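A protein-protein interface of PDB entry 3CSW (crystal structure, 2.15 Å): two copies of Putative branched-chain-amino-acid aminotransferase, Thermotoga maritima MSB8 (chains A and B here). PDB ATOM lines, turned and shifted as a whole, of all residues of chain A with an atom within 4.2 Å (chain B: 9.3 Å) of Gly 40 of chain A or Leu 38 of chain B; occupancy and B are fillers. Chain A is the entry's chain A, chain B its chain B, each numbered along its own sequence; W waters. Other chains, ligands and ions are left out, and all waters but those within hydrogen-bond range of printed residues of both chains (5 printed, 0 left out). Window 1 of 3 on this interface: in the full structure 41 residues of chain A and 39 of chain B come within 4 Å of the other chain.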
ATOM      1  N   SER A  37      12.537 -25.392 -25.513  1.00  0.00           N
ATOM      2  CA  SER A  37      11.400 -24.811 -26.217  1.00  0.00           C
ATOM      3  C   SER A  37      11.560 -23.310 -26.470  1.00  0.00           C
ATOM      4  O   SER A  37      10.819 -22.741 -27.255  1.00  0.00           O
ATOM      5  CB  SER A  37      10.086 -25.089 -25.448  1.00  0.00           C
ATOM      6  OG  SER A  37       9.984 -24.311 -24.248  1.00  0.00           O
ATOM      7  N   LEU A  38      12.508 -22.676 -25.786  1.00  0.00           N
ATOM      8  CA  LEU A  38      12.838 -21.263 -25.991  1.00  0.00           C
ATOM      9  C   LEU A  38      13.446 -21.044 -27.371  1.00  0.00           C
ATOM     10  O   LEU A  38      13.427 -19.939 -27.881  1.00  0.00           O
ATOM     11  CB  LEU A  38      13.779 -20.746 -24.892  1.00  0.00           C
ATOM     12  CG  LEU A  38      13.267 -20.790 -23.441  1.00  0.00           C
ATOM     13  CD1 LEU A  38      14.296 -20.169 -22.479  1.00  0.00           C
ATOM     14  CD2 LEU A  38      11.921 -20.102 -23.293  1.00  0.00           C
ATOM     15  N   GLN A  39      13.966 -22.114 -27.972  1.00  0.00           N
ATOM     16  CA  GLN A  39      14.434 -22.100 -29.358  1.00  0.00           C
ATOM     17  C   GLN A  39      13.299 -22.153 -30.386  1.00  0.00           C
ATOM     18  O   GLN A  39      13.551 -22.001 -31.586  1.00  0.00           O
ATOM     19  CB  GLN A  39      15.405 -23.264 -29.611  1.00  0.00           C
ATOM     20  CG  GLN A  39      16.630 -23.194 -28.700  1.00  0.00           C
ATOM     21  CD  GLN A  39      17.705 -24.237 -29.002  1.00  0.00           C
ATOM     22  OE1 GLN A  39      18.107 -24.972 -28.115  1.00  0.00           O
ATOM     23  NE2 GLN A  39      18.188 -24.279 -30.245  1.00  0.00           N
ATOM     24  N   GLY A  40      12.071 -22.413 -29.917  1.00  0.00           N
ATOM     25  CA  GLY A  40      10.891 -22.438 -30.755  1.00  0.00           C
ATOM     26  C   GLY A  40      10.223 -23.807 -30.868  1.00  0.00           C
ATOM     27  O   GLY A  40      10.873 -24.834 -30.777  1.00  0.00           O
ATOM     28  N   ALA A  41       8.904 -23.799 -31.044  1.00  0.00           N
ATOM     29  CA  ALA A  41       8.142 -24.995 -31.370  1.00  0.00           C
ATOM     30  C   ALA A  41       7.557 -24.835 -32.767  1.00  0.00           C
ATOM     31  O   ALA A  41       7.147 -23.737 -33.144  1.00  0.00           O
ATOM     32  CB  ALA A  41       7.015 -25.203 -30.364  1.00  0.00           C
ATOM     33  N   TYR A 101       1.258 -27.479 -31.142  1.00  0.00           N
ATOM     34  CA  TYR A 101       2.685 -27.237 -31.031  1.00  0.00           C
ATOM     35  C   TYR A 101       3.448 -28.538 -30.996  1.00  0.00           C
ATOM     36  O   TYR A 101       3.087 -29.443 -30.246  1.00  0.00           O
ATOM     37  CB  TYR A 101       2.997 -26.476 -29.751  1.00  0.00           C
ATOM     38  CG  TYR A 101       2.360 -25.103 -29.633  1.00  0.00           C
ATOM     39  CD1 TYR A 101       2.914 -23.998 -30.249  1.00  0.00           C
ATOM     40  CD2 TYR A 101       1.234 -24.906 -28.839  1.00  0.00           C
ATOM     41  CE1 TYR A 101       2.341 -22.732 -30.103  1.00  0.00           C
ATOM     42  CE2 TYR A 101       0.652 -23.660 -28.697  1.00  0.00           C
ATOM     43  CZ  TYR A 101       1.212 -22.579 -29.324  1.00  0.00           C
ATOM     44  OH  TYR A 101       0.632 -21.353 -29.164  1.00  0.00           O
ATOM     45  N   PHE A 103       7.188 -30.062 -30.179  1.00  0.00           N
ATOM     46  CA  PHE A 103       8.377 -29.652 -29.434  1.00  0.00           C
ATOM     47  C   PHE A 103       9.659 -30.345 -29.848  1.00  0.00           C
ATOM     48  O   PHE A 103       9.652 -31.538 -30.175  1.00  0.00           O
ATOM     49  CB  PHE A 103       8.158 -29.762 -27.915  1.00  0.00           C
ATOM     50  CG  PHE A 103       7.190 -28.751 -27.396  1.00  0.00           C
ATOM     51  CD1 PHE A 103       7.563 -27.425 -27.271  1.00  0.00           C
ATOM     52  CD2 PHE A 103       5.888 -29.106 -27.099  1.00  0.00           C
ATOM     53  CE1 PHE A 103       6.660 -26.482 -26.834  1.00  0.00           C
ATOM     54  CE2 PHE A 103       4.987 -28.169 -26.657  1.00  0.00           C
ATOM     55  CZ  PHE A 103       5.371 -26.853 -26.529  1.00  0.00           C
ATOM     56  N   PRO A 104      10.775 -29.572 -29.786  1.00  0.00           N
ATOM     57  CA  PRO A 104      12.097 -29.935 -30.302  1.00  0.00           C
ATOM     58  C   PRO A 104      12.705 -31.119 -29.590  1.00  0.00           C
ATOM     59  O   PRO A 104      12.700 -31.171 -28.349  1.00  0.00           O
ATOM     60  CB  PRO A 104      12.954 -28.681 -30.053  1.00  0.00           C
ATOM     61  CG  PRO A 104      12.215 -27.861 -29.039  1.00  0.00           C
ATOM     62  CD  PRO A 104      10.781 -28.238 -29.132  1.00  0.00           C
ATOM     63  N   ILE A 146       7.499 -21.751 -37.206  1.00  0.00           N
ATOM     64  CA  ILE A 146       8.159 -21.928 -35.923  1.00  0.00           C
ATOM     65  C   ILE A 146       7.846 -20.678 -35.053  1.00  0.00           C
ATOM     66  O   ILE A 146       7.741 -19.562 -35.569  1.00  0.00           O
ATOM     67  CB  ILE A 146       9.660 -22.281 -36.093  1.00  0.00           C
ATOM     68  CG1 ILE A 146      10.231 -22.797 -34.761  1.00  0.00           C
ATOM     69  CG2 ILE A 146      10.480 -21.084 -36.659  1.00  0.00           C
ATOM     70  CD1 ILE A 146      11.484 -23.608 -34.886  1.00  0.00           C
ATOM     71  N   THR A 147       7.600 -20.894 -33.763  1.00  0.00           N
ATOM     72  CA  THR A 147       7.069 -19.849 -32.871  1.00  0.00           C
ATOM     73  C   THR A 147       8.012 -18.648 -32.649  1.00  0.00           C
ATOM     74  O   THR A 147       7.559 -17.530 -32.364  1.00  0.00           O
ATOM     75  CB  THR A 147       6.692 -20.429 -31.480  1.00  0.00           C
ATOM     76  OG1 THR A 147       7.813 -21.161 -30.953  1.00  0.00           O
ATOM     77  CG2 THR A 147       5.427 -21.329 -31.568  1.00  0.00           C
ATOM     78  N   GLY A 148       9.312 -18.883 -32.782  1.00  0.00           N
ATOM     79  CA  GLY A 148      10.299 -17.842 -32.543  1.00  0.00           C
ATOM     80  C   GLY A 148      10.888 -17.132 -33.735  1.00  0.00           C
ATOM     81  O   GLY A 148      11.753 -16.295 -33.541  1.00  0.00           O
ATOM     82  N   LEU B  29       4.453 -23.705 -14.734  1.00  0.00           N
ATOM     83  CA  LEU B  29       4.406 -22.344 -15.242  1.00  0.00           C
ATOM     84  C   LEU B  29       2.987 -21.934 -15.455  1.00  0.00           C
ATOM     85  O   LEU B  29       2.131 -22.771 -15.744  1.00  0.00           O
ATOM     86  CB  LEU B  29       5.091 -22.246 -16.613  1.00  0.00           C
ATOM     87  CG  LEU B  29       6.571 -22.548 -16.731  1.00  0.00           C
ATOM     88  CD1 LEU B  29       6.918 -22.734 -18.197  1.00  0.00           C
ATOM     89  CD2 LEU B  29       7.370 -21.422 -16.098  1.00  0.00           C
ATOM     90  N   PHE B  31       0.304 -21.043 -17.696  1.00  0.00           N
ATOM     91  CA  PHE B  31       0.233 -21.586 -19.044  1.00  0.00           C
ATOM     92  C   PHE B  31       0.424 -20.532 -20.125  1.00  0.00           C
ATOM     93  O   PHE B  31       1.124 -20.768 -21.099  1.00  0.00           O
ATOM     94  CB  PHE B  31      -1.069 -22.330 -19.309  1.00  0.00           C
ATOM     95  CG  PHE B  31      -1.169 -22.824 -20.711  1.00  0.00           C
ATOM     96  CD1 PHE B  31      -0.451 -23.939 -21.109  1.00  0.00           C
ATOM     97  CD2 PHE B  31      -1.909 -22.138 -21.652  1.00  0.00           C
ATOM     98  CE1 PHE B  31      -0.500 -24.377 -22.419  1.00  0.00           C
ATOM     99  CE2 PHE B  31      -1.970 -22.576 -22.945  1.00  0.00           C
ATOM    100  CZ  PHE B  31      -1.263 -23.693 -23.333  1.00  0.00           C
ATOM    101  N   SER B  32      -0.195 -19.371 -19.962  1.00  0.00           N
ATOM    102  CA  SER B  32      -0.062 -18.331 -20.978  1.00  0.00           C
ATOM    103  C   SER B  32       1.367 -17.747 -21.012  1.00  0.00           C
ATOM    104  O   SER B  32       1.837 -17.349 -22.082  1.00  0.00           O
ATOM    105  CB  SER B  32      -1.145 -17.253 -20.819  1.00  0.00           C
ATOM    106  OG  SER B  32      -0.845 -16.378 -19.760  1.00  0.00           O
ATOM    107  N   LEU B  33       2.055 -17.710 -19.863  1.00  0.00           N
ATOM    108  CA  LEU B  33       3.484 -17.358 -19.836  1.00  0.00           C
ATOM    109  C   LEU B  33       4.265 -18.344 -20.701  1.00  0.00           C
ATOM    110  O   LEU B  33       5.099 -17.936 -21.503  1.00  0.00           O
ATOM    111  CB  LEU B  33       4.077 -17.346 -18.404  1.00  0.00           C
ATOM    112  CG  LEU B  33       5.599 -17.038 -18.259  1.00  0.00           C
ATOM    113  CD1 LEU B  33       5.952 -16.340 -16.934  1.00  0.00           C
ATOM    114  CD2 LEU B  33       6.492 -18.274 -18.435  1.00  0.00           C
ATOM    115  N   PHE B  34       3.993 -19.639 -20.523  1.00  0.00           N
ATOM    116  CA  PHE B  34       4.680 -20.688 -21.280  1.00  0.00           C
ATOM    117  C   PHE B  34       4.503 -20.489 -22.784  1.00  0.00           C
ATOM    118  O   PHE B  34       5.468 -20.528 -23.545  1.00  0.00           O
ATOM    119  CB  PHE B  34       4.193 -22.085 -20.875  1.00  0.00           C
ATOM    120  CG  PHE B  34       4.712 -23.185 -21.765  1.00  0.00           C
ATOM    121  CD1 PHE B  34       6.065 -23.510 -21.774  1.00  0.00           C
ATOM    122  CD2 PHE B  34       3.858 -23.877 -22.611  1.00  0.00           C
ATOM    123  CE1 PHE B  34       6.555 -24.517 -22.604  1.00  0.00           C
ATOM    124  CE2 PHE B  34       4.343 -24.893 -23.433  1.00  0.00           C
ATOM    125  CZ  PHE B  34       5.694 -25.208 -23.425  1.00  0.00           C
ATOM    126  N   GLU B  35       3.258 -20.275 -23.181  1.00  0.00           N
ATOM    127  CA  GLU B  35       2.889 -20.071 -24.574  1.00  0.00           C
ATOM    128  C   GLU B  35       3.645 -18.873 -25.155  1.00  0.00           C
ATOM    129  O   GLU B  35       4.168 -18.925 -26.268  1.00  0.00           O
ATOM    130  CB  GLU B  35       1.365 -19.867 -24.675  1.00  0.00           C
ATOM    131  CG  GLU B  35       0.734 -20.424 -25.934  1.00  0.00           C
ATOM    132  CD  GLU B  35      -0.796 -20.498 -25.880  1.00  0.00           C
ATOM    133  OE1 GLU B  35      -1.415 -19.934 -24.944  1.00  0.00           O
ATOM    134  OE2 GLU B  35      -1.370 -21.129 -26.805  1.00  0.00           O
ATOM    135  N   LYS B  36       3.716 -17.798 -24.385  1.00  0.00           N
ATOM    136  CA  LYS B  36       4.411 -16.602 -24.820  1.00  0.00           C
ATOM    137  C   LYS B  36       5.953 -16.800 -24.814  1.00  0.00           C
ATOM    138  O   LYS B  36       6.669 -16.235 -25.644  1.00  0.00           O
ATOM    139  CB  LYS B  36       3.996 -15.432 -23.931  1.00  0.00           C
ATOM    140  CG  LYS B  36       4.423 -14.082 -24.449  1.00  0.00           C
ATOM    141  CD  LYS B  36       3.646 -12.949 -23.766  1.00  0.00           C
ATOM    142  CE  LYS B  36       4.542 -11.719 -23.537  1.00  0.00           C
ATOM    143  NZ  LYS B  36       5.141 -11.238 -24.797  1.00  0.00           N
ATOM    144  N   SER B  37       6.448 -17.634 -23.906  1.00  0.00           N
ATOM    145  CA  SER B  37       7.876 -17.907 -23.832  1.00  0.00           C
ATOM    146  C   SER B  37       8.375 -18.592 -25.124  1.00  0.00           C
ATOM    147  O   SER B  37       9.545 -18.493 -25.469  1.00  0.00           O
ATOM    148  CB  SER B  37       8.212 -18.734 -22.570  1.00  0.00           C
ATOM    149  OG  SER B  37       7.987 -20.136 -22.729  1.00  0.00           O
ATOM    150  N   LEU B  38       7.470 -19.284 -25.831  1.00  0.00           N
ATOM    151  CA  LEU B  38       7.789 -19.947 -27.105  1.00  0.00           C
ATOM    152  C   LEU B  38       8.209 -18.989 -28.226  1.00  0.00           C
ATOM    153  O   LEU B  38       8.795 -19.418 -29.214  1.00  0.00           O
ATOM    154  CB  LEU B  38       6.602 -20.800 -27.580  1.00  0.00           C
ATOM    155  CG  LEU B  38       6.170 -21.951 -26.667  1.00  0.00           C
ATOM    156  CD1 LEU B  38       4.969 -22.752 -27.265  1.00  0.00           C
ATOM    157  CD2 LEU B  38       7.374 -22.838 -26.374  1.00  0.00           C
ATOM    158  N   GLN B  39       7.915 -17.702 -28.058  1.00  0.00           N
ATOM    159  CA  GLN B  39       8.354 -16.659 -28.978  1.00  0.00           C
ATOM    160  C   GLN B  39       9.794 -16.230 -28.749  1.00  0.00           C
ATOM    161  O   GLN B  39      10.306 -15.453 -29.520  1.00  0.00           O
ATOM    162  CB  GLN B  39       7.441 -15.432 -28.859  1.00  0.00           C
ATOM    163  CG  GLN B  39       6.069 -15.688 -29.428  1.00  0.00           C
ATOM    164  CD  GLN B  39       5.220 -14.437 -29.473  1.00  0.00           C
ATOM    165  OE1 GLN B  39       4.829 -13.913 -28.433  1.00  0.00           O
ATOM    166  NE2 GLN B  39       4.934 -13.947 -30.687  1.00  0.00           N
ATOM    167  N   GLY B  40      10.417 -16.686 -27.665  1.00  0.00           N
ATOM    168  CA  GLY B  40      11.824 -16.416 -27.414  1.00  0.00           C
ATOM    169  C   GLY B  40      12.121 -15.581 -26.191  1.00  0.00           C
ATOM    170  O   GLY B  40      11.264 -14.853 -25.696  1.00  0.00           O
ATOM    171  N   ALA B  41      13.341 -15.739 -25.687  1.00  0.00           N
ATOM    172  CA  ALA B  41      13.866 -14.936 -24.588  1.00  0.00           C
ATOM    173  C   ALA B  41      15.158 -14.235 -25.030  1.00  0.00           C
ATOM    174  O   ALA B  41      15.920 -14.775 -25.843  1.00  0.00           O
ATOM    175  CB  ALA B  41      14.144 -15.817 -23.349  1.00  0.00           C
ATOM    176  N   PHE B 103      12.605 -12.290 -20.368  1.00  0.00           N
ATOM    177  CA  PHE B 103      11.406 -12.489 -21.186  1.00  0.00           C
ATOM    178  C   PHE B 103      10.721 -11.187 -21.563  1.00  0.00           C
ATOM    179  O   PHE B 103      10.397 -10.393 -20.687  1.00  0.00           O
ATOM    180  CB  PHE B 103      10.430 -13.418 -20.468  1.00  0.00           C
ATOM    181  CG  PHE B 103      10.950 -14.813 -20.318  1.00  0.00           C
ATOM    182  CD1 PHE B 103      10.681 -15.781 -21.276  1.00  0.00           C
ATOM    183  CD2 PHE B 103      11.757 -15.158 -19.229  1.00  0.00           C
ATOM    184  CE1 PHE B 103      11.190 -17.084 -21.138  1.00  0.00           C
ATOM    185  CE2 PHE B 103      12.274 -16.461 -19.093  1.00  0.00           C
ATOM    186  CZ  PHE B 103      11.981 -17.415 -20.045  1.00  0.00           C
ATOM    187  N   PRO B 104      10.537 -10.942 -22.871  1.00  0.00           N
ATOM    188  CA  PRO B 104       9.880  -9.722 -23.312  1.00  0.00           C
ATOM    189  C   PRO B 104       8.509  -9.512 -22.691  1.00  0.00           C
ATOM    190  O   PRO B 104       7.760 -10.476 -22.466  1.00  0.00           O
ATOM    191  CB  PRO B 104       9.750  -9.915 -24.827  1.00  0.00           C
ATOM    192  CG  PRO B 104      10.870 -10.807 -25.176  1.00  0.00           C
ATOM    193  CD  PRO B 104      10.976 -11.756 -24.018  1.00  0.00           C
ATOM    194  N   ILE B 146      18.265 -13.206 -29.201  1.00  0.00           N
ATOM    195  CA  ILE B 146      16.954 -13.768 -28.881  1.00  0.00           C
ATOM    196  C   ILE B 146      17.044 -15.265 -29.210  1.00  0.00           C
ATOM    197  O   ILE B 146      17.572 -15.654 -30.268  1.00  0.00           O
ATOM    198  CB  ILE B 146      15.793 -12.996 -29.623  1.00  0.00           C
ATOM    199  CG1 ILE B 146      14.420 -13.402 -29.059  1.00  0.00           C
ATOM    200  CG2 ILE B 146      15.933 -13.090 -31.186  1.00  0.00           C
ATOM    201  CD1 ILE B 146      13.250 -12.426 -29.378  1.00  0.00           C
ATOM    202  N   THR B 147      16.570 -16.100 -28.283  1.00  0.00           N
ATOM    203  CA  THR B 147      16.736 -17.568 -28.373  1.00  0.00           C
ATOM    204  C   THR B 147      16.129 -18.250 -29.595  1.00  0.00           C
ATOM    205  O   THR B 147      16.567 -19.336 -29.946  1.00  0.00           O
ATOM    206  CB  THR B 147      16.174 -18.285 -27.131  1.00  0.00           C
ATOM    207  OG1 THR B 147      14.809 -17.899 -26.947  1.00  0.00           O
ATOM    208  CG2 THR B 147      16.951 -17.921 -25.906  1.00  0.00           C
ATOM    209  N   GLY B 148      15.138 -17.637 -30.240  1.00  0.00           N
ATOM    210  CA  GLY B 148      14.461 -18.257 -31.372  1.00  0.00           C
ATOM    211  C   GLY B 148      14.940 -17.866 -32.761  1.00  0.00           C
ATOM    212  O   GLY B 148      14.417 -18.358 -33.747  1.00  0.00           O
ATOM    213  N   ARG B 149      15.937 -16.991 -32.846  1.00  0.00           N
ATOM    214  CA  ARG B 149      16.427 -16.519 -34.138  1.00  0.00           C
ATOM    215  C   ARG B 149      16.850 -17.719 -35.007  1.00  0.00           C
ATOM    216  O   ARG B 149      17.651 -18.567 -34.597  1.00  0.00           O
ATOM    217  CB  ARG B 149      17.481 -15.391 -34.015  1.00  0.00           C
ATOM    218  CG  ARG B 149      18.804 -15.700 -33.333  1.00  0.00           C
ATOM    219  CD  ARG B 149      19.695 -14.429 -33.335  1.00  0.00           C
ATOM    220  NE  ARG B 149      19.968 -14.046 -34.704  1.00  0.00           N
ATOM    221  CZ  ARG B 149      20.040 -12.800 -35.168  1.00  0.00           C
ATOM    222  NH1 ARG B 149      19.883 -11.732 -34.380  1.00  0.00           N
ATOM    223  NH2 ARG B 149      20.237 -12.626 -36.458  1.00  0.00           N
ATOM    224  N   THR B 150      16.243 -17.794 -36.190  1.00  0.00           N
ATOM    225  CA  THR B 150      16.287 -19.015 -36.997  1.00  0.00           C
ATOM    226  C   THR B 150      17.606 -19.255 -37.729  1.00  0.00           C
ATOM    227  O   THR B 150      17.912 -20.384 -38.095  1.00  0.00           O
ATOM    228  CB  THR B 150      15.104 -19.109 -37.942  1.00  0.00           C
ATOM    229  OG1 THR B 150      14.944 -17.870 -38.667  1.00  0.00           O
ATOM    230  CG2 THR B 150      13.825 -19.451 -37.169  1.00  0.00           C
ATOM    231  N   VAL B 153      19.407 -21.028 -34.813  1.00  0.00           N
ATOM    232  CA  VAL B 153      18.711 -22.289 -34.558  1.00  0.00           C
ATOM    233  C   VAL B 153      18.978 -23.331 -35.651  1.00  0.00           C
ATOM    234  O   VAL B 153      19.284 -24.481 -35.339  1.00  0.00           O
ATOM    235  CB  VAL B 153      17.176 -22.085 -34.275  1.00  0.00           C
ATOM    236  CG1 VAL B 153      16.404 -23.416 -34.335  1.00  0.00           C
ATOM    237  CG2 VAL B 153      16.993 -21.388 -32.911  1.00  0.00           C
ATOM    238  N   ARG B 157      21.846 -27.053 -36.063  1.00  0.00           N
ATOM    239  CA  ARG B 157      21.480 -28.424 -36.452  1.00  0.00           C
ATOM    240  C   ARG B 157      22.438 -29.017 -37.480  1.00  0.00           C
ATOM    241  O   ARG B 157      22.385 -30.206 -37.758  1.00  0.00           O
ATOM    242  CB  ARG B 157      20.053 -28.504 -37.017  1.00  0.00           C
ATOM    243  CG  ARG B 157      18.975 -27.624 -36.346  1.00  0.00           C
ATOM    244  CD  ARG B 157      18.619 -27.956 -34.887  1.00  0.00           C
ATOM    245  NE  ARG B 157      17.793 -29.167 -34.748  1.00  0.00           N
ATOM    246  CZ  ARG B 157      16.948 -29.429 -33.738  1.00  0.00           C
ATOM    247  NH1 ARG B 157      16.733 -28.563 -32.737  1.00  0.00           N
ATOM    248  NH2 ARG B 157      16.281 -30.576 -33.741  1.00  0.00           N
HETATM  249  O   HOH W   1      12.786 -15.745 -30.997  1.00  0.00           O
HETATM  250  O   HOH W   2      11.561 -19.135 -29.794  1.00  0.00           O
HETATM  251  O   HOH W   3      16.085 -26.060 -31.095  1.00  0.00           O
HETATM  252  O   HOH W   4      18.822 -25.666 -32.872  1.00  0.00           O
HETATM  253  O   HOH W   5      12.288 -20.240 -33.426  1.00  0.00           O
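The backbone carbonyl oxygen (O) of Leu 38 of chain A lies within hydrogen-bond range of the side-chain hydroxyl (OG1) of Thr 147 of chain B, at 2.6 Å. The side-chain carboxylate of Glu 35 of chain B lies within hydrogen-bond range of the side-chain hydroxyl of Tyr 101 of chain A, 3.1 Å away. O of Leu 38 of chain B is in hydrogen-bond range of OG1 of Thr 147 of chain A (2.7 Å). The backbone carbonyl oxygen (O) of Gly 148 of chain A sits close to the backbone carbonyl oxygen (O) of Gly 148 of chain B (3.4 Å).
N of Ala 41 of chain A sits at hydrogen-bond distance from OG1 of Thr 147 of chain A, 2.9 Å away. O of Phe 34 of chain B lies within hydrogen-bond range of OG of Ser 37 of chain B (2.7 Å). The backbone carbonyl oxygen of Ala 41 of chain B is in hydrogen-bond range of the backbone NH of Thr 147 of chain B, at 2.9 Å.
Among the printed residues, merely in contact across the chains: Phe 103 of chain A with Phe 34 of chain B (3.5 Å), Gln 39 of chain A with Thr 147 of chain B (3.5 Å), Ser 37 of chain A with Leu 38 of chain B (3.6 Å), Thr 147 of chain A with Gln 39 of chain B (3.6 Å), Leu 38 of chain A with Ser 37 of chain B (3.6 Å), Gly 148 of chain A with Leu 38 of chain B (3.6 Å), Leu 38 of chain A with Gly 148 of chain B (3.7 Å), Gln 39 of chain A with Val 153 of chain B (3.7 Å), Phe 103 of chain A with Leu 38 of chain B (3.7 Å), Ile 146 of chain A with Thr 150 of chain B (3.8 Å), Leu 38 of chain A with Phe 103 of chain B (3.8 Å), Ser 37 of chain A with Phe 34 of chain B (3.8 Å), Tyr 101 of chain A with Leu 38 of chain B (3.8 Å), Gly 148 of chain A with Gln 39 of chain B (3.9 Å), Gln 39 of chain A with Gly 148 of chain B (3.9 Å), Leu 38 of chain A with Gly 40 of chain B (3.9 Å) and Gly 40 of chain A with Leu 38 of chain B (3.99 Å).
Printed residues of chain B within 4 Å of Leu 38 of chain A: Ser 37, Gly 40, Phe 103, Thr 147 and Gly 148. Printed residues of chain B within 4 Å of Gly 40 of chain A: Leu 38. No residue of chain B comes within 4 Å of Ala 41 of chain A. Printed residues of chain B within 4 Å of Tyr 101 of chain A: Glu 35 (3.1 Å) and Leu 38 (3.8 Å). Of chain B, only Leu 38 and Gln 39 come within 4 Å of Thr 147 of chain A. Of the printed residues of chain A, Glu 35 of chain B touches Tyr 101 (3.1 Å). Of the printed residues of chain A, Thr 150 of chain B touches Ile 146 (3.8 Å). The nearest printed residue of chain A that does not touch Leu 38 of chain B is Ala 41 of chain A (4.4 Å).
Printed residues of chain B that touch a printed residue of chain A: Phe 34, Glu 35, Ser 37, Leu 38, Gln 39, Gly 40, Phe 103, Thr 147, Gly 148, Thr 150 and Val 153. Hydrophobic or aromatic side chains of chain B within 4 Å of the printed part of chain A: Phe 34, Leu 38, Phe 103 and Val 153. Hydrophobic or aromatic side chains of chain A within 4 Å of the printed part of chain B: Leu 38, Tyr 101, Phe 103 and Ile 146. Among the printed residues, 21 pairs touch across the chains. Among the printed residues, no Asp or Glu carboxylate lies within 4 Å of a Lys or Arg side-chain nitrogen of the other chain.
Ser 37 of chain A touches Leu 38 of chain B, and with the chains exchanged Leu 38 of chain A touches Ser 37 of chain B. Leu 38 of chain A touches Thr 147 of chain B, and with the chains exchanged Thr 147 of chain A touches Leu 38 of chain B. Leu 38 of chain A touches Gly 148 of chain B, and with the chains exchanged Gly 148 of chain A touches Leu 38 of chain B. Gln 39 of chain A touches Thr 147 of chain B, and with the chains exchanged Thr 147 of chain A touches Gln 39 of chain B. Positions printed for both chains: 37, 38, 39, 40, 41, 103, 104, 146, 147 and 148. Of the 21 pairs that touch across the chains among the printed residues, 15 have their exchanged pair printed and touching as well.
Water W4 bridges O of Val 153 of chain B (2.8 Å) and NE2 of Gln 39 of chain A (3.0 Å). Water W2 lies within hydrogen-bond range of the backbone carbonyl oxygen (O) of Leu 38 of chain A (2.8 Å), the backbone carbonyl oxygen (O) of Leu 38 of chain B (2.8 Å), the backbone NH (N) of Gly 40 of chain A (3.3 Å) and the backbone NH (N) of Gly 40 of chain B (3.4 Å). Water W1 lies within hydrogen-bond range of the backbone carbonyl oxygen of Gly 148 of chain A (2.8 Å), the backbone carbonyl oxygen of Gln 39 of chain B (2.9 Å) and the backbone NH of Gly 148 of chain B (3.1 Å). Water W5 lies within hydrogen-bond range of the backbone carbonyl oxygen of Gln 39 of chain A (2.8 Å), the backbone carbonyl oxygen of Gly 148 of chain B (2.9 Å) and the backbone NH of Gly 148 of chain A (3.3 Å). Water W3 lies within hydrogen-bond range of the side-chain amide nitrogen of Gln 39 of chain A (2.9 Å) and the guanidinium group of Arg 157 of chain B (3.1 Å).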
